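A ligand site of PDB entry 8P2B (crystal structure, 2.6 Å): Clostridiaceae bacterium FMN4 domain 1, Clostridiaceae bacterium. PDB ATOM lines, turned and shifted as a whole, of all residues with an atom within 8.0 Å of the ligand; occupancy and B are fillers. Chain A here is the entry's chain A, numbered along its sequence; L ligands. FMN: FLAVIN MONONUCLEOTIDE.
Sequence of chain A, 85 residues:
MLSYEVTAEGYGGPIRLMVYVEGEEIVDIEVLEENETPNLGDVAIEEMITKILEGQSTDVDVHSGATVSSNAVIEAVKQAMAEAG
Residues that only touch the ligand: Tyr 11 (3.2 Å), Gly 65 (3.5 Å), Leu 40 (3.6 Å), Gly 41 (3.6 Å) and Glu 36 (3.9 Å).
Of the 27 residues printed, 11 come within 4 Å of the ligand.
The nearest printed residue that does not touch the ligand is Val 62 (4.4 Å).
O of Thr 67 sits close to ND2 of Asn 71 (3.4 Å).
OG of Ser 69 is in hydrogen-bond range of OE2 of Glu 36 (2.6 Å).
The side-chain hydroxyl of Ser 70 is in hydrogen-bond range of the backbone carbonyl oxygen of Ala 66.
N of Tyr 11 is in hydrogen-bond range of OE2 of Glu 36, at 2.6 Å.
The backbone NH (N) of Leu 40 lies within hydrogen-bond range of the side-chain carboxylate (OD1) of Asp 42 (3.5 Å).
OE1 of Glu 36 sits at hydrogen-bond distance from N of Gly 12.
The backbone NH (N) of Glu 36 lies within hydrogen-bond range of the side-chain carboxylate (OE1) of Glu 34.
The backbone NH (N) of Thr 67 sits at hydrogen-bond distance from an oxygen (O5') of the ligand (2.9 Å).
P of the ligand is covalently linked to OG1 of Thr 67, 1.6 Å away.
The backbone carbonyl oxygen (O) of Ser 64 lies close to an oxygen (O1P) of the ligand, at 2.4 Å.
The backbone NH (N) of Ser 69 is in hydrogen-bond range of an oxygen (O2) of the ligand, at 2.8 Å.
OG of Ser 69 sits at hydrogen-bond distance from N3 of the ligand (3.0 Å).
O4 of the ligand is in hydrogen-bond range of N of Thr 37, at 3.1 Å.
OG1 of Thr 37 is in hydrogen-bond range of N5 of the ligand (2.9 Å).
An oxygen (O2) of the ligand sits at hydrogen-bond distance from the backbone NH of Val 68, at 3.0 Å.
O5' of the ligand sits at hydrogen-bond distance from N of Ala 66 (3.3 Å).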
ATOM      1  N   GLY A  10     -11.501  -5.826  21.416  1.00  0.00           N
ATOM      2  CA  GLY A  10     -11.928  -6.989  22.162  1.00  0.00           C
ATOM      3  C   GLY A  10     -12.078  -6.640  23.643  1.00  0.00           C
ATOM      4  O   GLY A  10     -12.048  -5.473  24.023  1.00  0.00           O
ATOM      5  N   TYR A  11     -12.210  -7.693  24.456  1.00  0.00           N
ATOM      6  CA  TYR A  11     -12.449  -7.582  25.885  1.00  0.00           C
ATOM      7  C   TYR A  11     -11.183  -7.138  26.598  1.00  0.00           C
ATOM      8  O   TYR A  11     -11.239  -6.380  27.561  1.00  0.00           O
ATOM      9  CB  TYR A  11     -13.001  -8.913  26.436  1.00  0.00           C
ATOM     10  CG  TYR A  11     -13.316  -8.922  27.911  1.00  0.00           C
ATOM     11  CD1 TYR A  11     -12.325  -9.155  28.855  1.00  0.00           C
ATOM     12  CD2 TYR A  11     -14.605  -8.644  28.375  1.00  0.00           C
ATOM     13  CE1 TYR A  11     -12.603  -9.162  30.218  1.00  0.00           C
ATOM     14  CE2 TYR A  11     -14.913  -8.642  29.735  1.00  0.00           C
ATOM     15  CZ  TYR A  11     -13.897  -8.900  30.648  1.00  0.00           C
ATOM     16  OH  TYR A  11     -14.199  -8.862  31.977  1.00  0.00           O
ATOM     17  N   GLY A  12     -10.036  -7.652  26.150  1.00  0.00           N
ATOM     18  CA  GLY A  12      -8.789  -7.429  26.858  1.00  0.00           C
ATOM     19  C   GLY A  12      -7.967  -6.308  26.223  1.00  0.00           C
ATOM     20  O   GLY A  12      -6.863  -6.014  26.678  1.00  0.00           O
ATOM     21  N   GLY A  13      -8.561  -5.655  25.226  1.00  0.00           N
ATOM     22  CA  GLY A  13      -7.888  -4.682  24.389  1.00  0.00           C
ATOM     23  C   GLY A  13      -8.062  -5.105  22.946  1.00  0.00           C
ATOM     24  O   GLY A  13      -8.667  -6.134  22.649  1.00  0.00           O
ATOM     25  N   GLU A  34      -3.834 -11.210  19.850  1.00  0.00           N
ATOM     26  CA  GLU A  34      -4.889 -10.999  20.830  1.00  0.00           C
ATOM     27  C   GLU A  34      -4.298 -11.110  22.235  1.00  0.00           C
ATOM     28  O   GLU A  34      -3.360 -11.871  22.474  1.00  0.00           O
ATOM     29  CB  GLU A  34      -6.071 -11.939  20.624  1.00  0.00           C
ATOM     30  CG  GLU A  34      -5.783 -13.405  20.861  1.00  0.00           C
ATOM     31  CD  GLU A  34      -5.485 -13.875  22.281  1.00  0.00           C
ATOM     32  OE1 GLU A  34      -6.198 -13.510  23.239  1.00  0.00           O
ATOM     33  OE2 GLU A  34      -4.548 -14.676  22.397  1.00  0.00           O
ATOM     34  N   ASN A  35      -4.877 -10.273  23.122  1.00  0.00           N
ATOM     35  CA  ASN A  35      -4.574 -10.298  24.545  1.00  0.00           C
ATOM     36  C   ASN A  35      -5.893 -10.393  25.309  1.00  0.00           C
ATOM     37  O   ASN A  35      -6.077  -9.700  26.306  1.00  0.00           O
ATOM     38  CB  ASN A  35      -3.670  -9.128  24.935  1.00  0.00           C
ATOM     39  CG  ASN A  35      -2.348  -9.247  24.207  1.00  0.00           C
ATOM     40  OD1 ASN A  35      -2.105  -8.487  23.282  1.00  0.00           O
ATOM     41  ND2 ASN A  35      -1.618 -10.317  24.482  1.00  0.00           N
ATOM     42  N   GLU A  36      -6.769 -11.293  24.848  1.00  0.00           N
ATOM     43  CA  GLU A  36      -7.976 -11.669  25.566  1.00  0.00           C
ATOM     44  C   GLU A  36      -7.617 -12.612  26.711  1.00  0.00           C
ATOM     45  O   GLU A  36      -6.481 -13.086  26.804  1.00  0.00           O
ATOM     46  CB  GLU A  36      -9.003 -12.356  24.666  1.00  0.00           C
ATOM     47  CG  GLU A  36      -9.387 -11.562  23.443  1.00  0.00           C
ATOM     48  CD  GLU A  36      -9.879 -10.149  23.734  1.00  0.00           C
ATOM     49  OE1 GLU A  36      -9.016  -9.242  23.959  1.00  0.00           O
ATOM     50  OE2 GLU A  36     -11.111  -9.973  23.733  1.00  0.00           O
ATOM     51  N   THR A  37      -8.627 -12.875  27.537  1.00  0.00           N
ATOM     52  CA  THR A  37      -8.497 -13.651  28.763  1.00  0.00           C
ATOM     53  C   THR A  37      -8.189 -15.111  28.406  1.00  0.00           C
ATOM     54  O   THR A  37      -8.976 -15.756  27.712  1.00  0.00           O
ATOM     55  CB  THR A  37      -9.775 -13.527  29.616  1.00  0.00           C
ATOM     56  OG1 THR A  37      -9.934 -12.208  30.132  1.00  0.00           O
ATOM     57  CG2 THR A  37      -9.745 -14.506  30.771  1.00  0.00           C
ATOM     58  N   PRO A  38      -7.018 -15.659  28.835  1.00  0.00           N
ATOM     59  CA  PRO A  38      -6.695 -17.069  28.554  1.00  0.00           C
ATOM     60  C   PRO A  38      -7.832 -18.015  28.955  1.00  0.00           C
ATOM     61  O   PRO A  38      -8.495 -17.788  29.978  1.00  0.00           O
ATOM     62  CB  PRO A  38      -5.436 -17.314  29.385  1.00  0.00           C
ATOM     63  CG  PRO A  38      -4.785 -15.951  29.498  1.00  0.00           C
ATOM     64  CD  PRO A  38      -5.927 -14.952  29.525  1.00  0.00           C
ATOM     65  N   ASN A  39      -8.071 -19.020  28.106  1.00  0.00           N
ATOM     66  CA  ASN A  39      -9.019 -20.107  28.327  1.00  0.00           C
ATOM     67  C   ASN A  39     -10.459 -19.617  28.216  1.00  0.00           C
ATOM     68  O   ASN A  39     -11.370 -20.356  28.594  1.00  0.00           O
ATOM     69  CB  ASN A  39      -8.781 -20.798  29.671  1.00  0.00           C
ATOM     70  CG  ASN A  39      -7.714 -21.856  29.615  1.00  0.00           C
ATOM     71  OD1 ASN A  39      -6.567 -21.624  30.012  1.00  0.00           O
ATOM     72  ND2 ASN A  39      -8.109 -23.040  29.157  1.00  0.00           N
ATOM     73  N   LEU A  40     -10.666 -18.416  27.691  1.00  0.00           N
ATOM     74  CA  LEU A  40     -12.007 -17.852  27.568  1.00  0.00           C
ATOM     75  C   LEU A  40     -12.133 -17.061  26.265  1.00  0.00           C
ATOM     76  O   LEU A  40     -12.883 -17.462  25.363  1.00  0.00           O
ATOM     77  CB  LEU A  40     -12.272 -17.027  28.844  1.00  0.00           C
ATOM     78  CG  LEU A  40     -13.458 -16.056  28.859  1.00  0.00           C
ATOM     79  CD1 LEU A  40     -14.681 -16.573  28.133  1.00  0.00           C
ATOM     80  CD2 LEU A  40     -13.850 -15.777  30.305  1.00  0.00           C
ATOM     81  N   GLY A  41     -11.378 -15.958  26.155  1.00  0.00           N
ATOM     82  CA  GLY A  41     -11.476 -15.075  24.998  1.00  0.00           C
ATOM     83  C   GLY A  41     -10.692 -15.619  23.814  1.00  0.00           C
ATOM     84  O   GLY A  41     -11.188 -15.574  22.697  1.00  0.00           O
ATOM     85  N   ASP A  42      -9.476 -16.134  24.062  1.00  0.00           N
ATOM     86  CA  ASP A  42      -8.637 -16.692  23.014  1.00  0.00           C
ATOM     87  C   ASP A  42      -9.343 -17.866  22.351  1.00  0.00           C
ATOM     88  O   ASP A  42      -9.294 -18.043  21.127  1.00  0.00           O
ATOM     89  CB  ASP A  42      -7.231 -17.049  23.516  1.00  0.00           C
ATOM     90  CG  ASP A  42      -7.122 -17.885  24.780  1.00  0.00           C
ATOM     91  OD1 ASP A  42      -8.162 -18.279  25.312  1.00  0.00           O
ATOM     92  OD2 ASP A  42      -5.974 -18.099  25.240  1.00  0.00           O
ATOM     93  N   VAL A  43     -10.024 -18.654  23.188  1.00  0.00           N
ATOM     94  CA  VAL A  43     -10.791 -19.802  22.754  1.00  0.00           C
ATOM     95  C   VAL A  43     -11.990 -19.368  21.904  1.00  0.00           C
ATOM     96  O   VAL A  43     -12.320 -20.022  20.906  1.00  0.00           O
ATOM     97  CB  VAL A  43     -11.235 -20.654  23.964  1.00  0.00           C
ATOM     98  CG1 VAL A  43     -12.203 -21.759  23.546  1.00  0.00           C
ATOM     99  CG2 VAL A  43     -10.051 -21.260  24.684  1.00  0.00           C
ATOM    100  N   ALA A  44     -12.677 -18.287  22.315  1.00  0.00           N
ATOM    101  CA  ALA A  44     -13.840 -17.789  21.594  1.00  0.00           C
ATOM    102  C   ALA A  44     -13.440 -17.364  20.183  1.00  0.00           C
ATOM    103  O   ALA A  44     -14.230 -17.474  19.250  1.00  0.00           O
ATOM    104  CB  ALA A  44     -14.469 -16.645  22.353  1.00  0.00           C
ATOM    105  N   ILE A  45     -12.213 -16.840  20.050  1.00  0.00           N
ATOM    106  CA  ILE A  45     -11.683 -16.360  18.784  1.00  0.00           C
ATOM    107  C   ILE A  45     -11.494 -17.569  17.875  1.00  0.00           C
ATOM    108  O   ILE A  45     -12.085 -17.565  16.796  1.00  0.00           O
ATOM    109  CB  ILE A  45     -10.404 -15.515  18.991  1.00  0.00           C
ATOM    110  CG1 ILE A  45     -10.698 -14.116  19.553  1.00  0.00           C
ATOM    111  CG2 ILE A  45      -9.580 -15.396  17.723  1.00  0.00           C
ATOM    112  CD1 ILE A  45      -9.476 -13.441  20.151  1.00  0.00           C
ATOM    113  N   VAL A  62     -22.390 -16.147  18.679  1.00  0.00           N
ATOM    114  CA  VAL A  62     -21.300 -15.889  19.600  1.00  0.00           C
ATOM    115  C   VAL A  62     -20.986 -17.170  20.367  1.00  0.00           C
ATOM    116  O   VAL A  62     -21.849 -17.986  20.576  1.00  0.00           O
ATOM    117  CB  VAL A  62     -21.620 -14.725  20.573  1.00  0.00           C
ATOM    118  CG1 VAL A  62     -21.607 -13.373  19.867  1.00  0.00           C
ATOM    119  CG2 VAL A  62     -22.937 -14.929  21.324  1.00  0.00           C
ATOM    120  N   HIS A  63     -19.736 -17.316  20.802  1.00  0.00           N
ATOM    121  CA  HIS A  63     -19.372 -18.205  21.883  1.00  0.00           C
ATOM    122  C   HIS A  63     -19.851 -17.598  23.198  1.00  0.00           C
ATOM    123  O   HIS A  63     -19.307 -16.584  23.647  1.00  0.00           O
ATOM    124  CB  HIS A  63     -17.845 -18.417  21.876  1.00  0.00           C
ATOM    125  CG  HIS A  63     -17.394 -19.708  22.478  1.00  0.00           C
ATOM    126  ND1 HIS A  63     -16.681 -19.785  23.663  1.00  0.00           N
ATOM    127  CD2 HIS A  63     -17.562 -20.962  22.021  1.00  0.00           C
ATOM    128  CE1 HIS A  63     -16.417 -21.059  23.918  1.00  0.00           C
ATOM    129  NE2 HIS A  63     -16.940 -21.792  22.924  1.00  0.00           N
ATOM    130  N   SER A  64     -20.800 -18.263  23.858  1.00  0.00           N
ATOM    131  CA  SER A  64     -21.705 -17.638  24.830  1.00  0.00           C
ATOM    132  C   SER A  64     -21.050 -17.126  26.104  1.00  0.00           C
ATOM    133  O   SER A  64     -21.587 -16.212  26.727  1.00  0.00           O
ATOM    134  CB  SER A  64     -22.824 -18.557  25.191  1.00  0.00           C
ATOM    135  OG  SER A  64     -23.746 -18.574  24.115  1.00  0.00           O
ATOM    136  N   GLY A  65     -19.904 -17.661  26.522  1.00  0.00           N
ATOM    137  CA  GLY A  65     -19.231 -17.085  27.683  1.00  0.00           C
ATOM    138  C   GLY A  65     -18.516 -15.761  27.383  1.00  0.00           C
ATOM    139  O   GLY A  65     -17.889 -15.191  28.260  1.00  0.00           O
ATOM    140  N   ALA A  66     -18.541 -15.318  26.128  1.00  0.00           N
ATOM    141  CA  ALA A  66     -17.477 -14.463  25.603  1.00  0.00           C
ATOM    142  C   ALA A  66     -18.011 -13.690  24.404  1.00  0.00           C
ATOM    143  O   ALA A  66     -17.446 -13.732  23.315  1.00  0.00           O
ATOM    144  CB  ALA A  66     -16.261 -15.285  25.208  1.00  0.00           C
ATOM    145  N   THR A  67     -19.090 -12.955  24.630  1.00  0.00           N
ATOM    146  CA  THR A  67     -19.714 -12.179  23.562  1.00  0.00           C
ATOM    147  C   THR A  67     -18.790 -11.064  23.070  1.00  0.00           C
ATOM    148  O   THR A  67     -18.904 -10.632  21.927  1.00  0.00           O
ATOM    149  CB  THR A  67     -21.056 -11.647  24.071  1.00  0.00           C
ATOM    150  OG1 THR A  67     -21.801 -12.846  24.276  1.00  0.00           O
ATOM    151  CG2 THR A  67     -21.784 -10.707  23.120  1.00  0.00           C
ATOM    152  N   VAL A  68     -17.891 -10.563  23.925  1.00  0.00           N
ATOM    153  CA  VAL A  68     -17.170  -9.359  23.563  1.00  0.00           C
ATOM    154  C   VAL A  68     -16.045  -9.725  22.582  1.00  0.00           C
ATOM    155  O   VAL A  68     -15.883  -9.053  21.554  1.00  0.00           O
ATOM    156  CB  VAL A  68     -16.659  -8.607  24.799  1.00  0.00           C
ATOM    157  CG1 VAL A  68     -15.745  -7.456  24.423  1.00  0.00           C
ATOM    158  CG2 VAL A  68     -17.821  -8.077  25.633  1.00  0.00           C
ATOM    159  N   SER A  69     -15.305 -10.801  22.910  1.00  0.00           N
ATOM    160  CA  SER A  69     -14.336 -11.422  22.013  1.00  0.00           C
ATOM    161  C   SER A  69     -15.018 -11.907  20.721  1.00  0.00           C
ATOM    162  O   SER A  69     -14.481 -11.789  19.623  1.00  0.00           O
ATOM    163  CB  SER A  69     -13.585 -12.547  22.706  1.00  0.00           C
ATOM    164  OG  SER A  69     -12.589 -12.048  23.583  1.00  0.00           O
ATOM    165  N   SER A  70     -16.222 -12.452  20.860  1.00  0.00           N
ATOM    166  CA  SER A  70     -16.894 -13.043  19.706  1.00  0.00           C
ATOM    167  C   SER A  70     -17.270 -11.945  18.716  1.00  0.00           C
ATOM    168  O   SER A  70     -16.987 -12.072  17.526  1.00  0.00           O
ATOM    169  CB  SER A  70     -18.079 -13.904  20.120  1.00  0.00           C
ATOM    170  OG  SER A  70     -17.629 -15.016  20.894  1.00  0.00           O
ATOM    171  N   ASN A  71     -17.889 -10.867  19.214  1.00  0.00           N
ATOM    172  CA  ASN A  71     -18.319  -9.758  18.390  1.00  0.00           C
ATOM    173  C   ASN A  71     -17.100  -9.050  17.784  1.00  0.00           C
ATOM    174  O   ASN A  71     -17.168  -8.566  16.674  1.00  0.00           O
ATOM    175  CB  ASN A  71     -19.163  -8.727  19.140  1.00  0.00           C
ATOM    176  CG  ASN A  71     -20.527  -9.211  19.582  1.00  0.00           C
ATOM    177  OD1 ASN A  71     -21.061 -10.193  19.089  1.00  0.00           O
ATOM    178  ND2 ASN A  71     -21.126  -8.514  20.529  1.00  0.00           N
ATOM    179  N   ALA A  72     -15.975  -8.999  18.506  1.00  0.00           N
ATOM    180  CA  ALA A  72     -14.774  -8.398  17.936  1.00  0.00           C
ATOM    181  C   ALA A  72     -14.404  -9.123  16.636  1.00  0.00           C
ATOM    182  O   ALA A  72     -14.080  -8.477  15.646  1.00  0.00           O
ATOM    183  CB  ALA A  72     -13.627  -8.422  18.911  1.00  0.00           C
HETATM  184  N1  FMN L   1     -15.702 -12.044  27.679  1.00  0.00           N
HETATM  185  C2  FMN L   1     -15.066 -12.078  26.489  1.00  0.00           C
HETATM  186  O2  FMN L   1     -15.700 -11.986  25.441  1.00  0.00           O
HETATM  187  N3  FMN L   1     -13.691 -12.194  26.414  1.00  0.00           N
HETATM  188  C4  FMN L   1     -12.901 -12.285  27.542  1.00  0.00           C
HETATM  189  O4  FMN L   1     -11.677 -12.396  27.440  1.00  0.00           O
HETATM  190  C4A FMN L   1     -13.551 -12.247  28.798  1.00  0.00           C
HETATM  191  N5  FMN L   1     -12.821 -12.350  29.888  1.00  0.00           N
HETATM  192  C5A FMN L   1     -13.474 -12.294  31.087  1.00  0.00           C
HETATM  193  C6  FMN L   1     -12.716 -12.373  32.275  1.00  0.00           C
HETATM  194  C7  FMN L   1     -13.309 -12.346  33.524  1.00  0.00           C
HETATM  195  C7M FMN L   1     -12.504 -12.532  34.787  1.00  0.00           C
HETATM  196  C8  FMN L   1     -14.722 -12.154  33.604  1.00  0.00           C
HETATM  197  C8M FMN L   1     -15.411 -12.100  34.940  1.00  0.00           C
HETATM  198  C9  FMN L   1     -15.478 -12.092  32.449  1.00  0.00           C
HETATM  199  C9A FMN L   1     -14.881 -12.154  31.177  1.00  0.00           C
HETATM  200  N10 FMN L   1     -15.614 -12.048  29.990  1.00  0.00           N
HETATM  201  C10 FMN L   1     -14.992 -12.133  28.774  1.00  0.00           C
HETATM  202  C1' FMN L   1     -17.094 -12.060  30.031  1.00  0.00           C
HETATM  203  C2' FMN L   1     -17.771 -10.739  29.961  1.00  0.00           C
HETATM  204  O2' FMN L   1     -17.702 -10.121  31.253  1.00  0.00           O
HETATM  205  C3' FMN L   1     -19.217 -11.020  29.515  1.00  0.00           C
HETATM  206  O3' FMN L   1     -19.958 -11.520  30.587  1.00  0.00           O
HETATM  207  C4' FMN L   1     -19.380 -12.041  28.389  1.00  0.00           C
HETATM  208  O4' FMN L   1     -18.451 -11.765  27.325  1.00  0.00           O
HETATM  209  C5' FMN L   1     -20.791 -12.055  27.851  1.00  0.00           C
HETATM  210  O5' FMN L   1     -20.926 -13.144  26.889  1.00  0.00           O
HETATM  211  P   FMN L   1     -22.155 -13.060  25.837  1.00  0.00           P
HETATM  212  O1P FMN L   1     -22.812 -14.423  25.684  1.00  0.00           O
HETATM  213  O2P FMN L   1     -23.130 -12.043  26.407  1.00  0.00           O
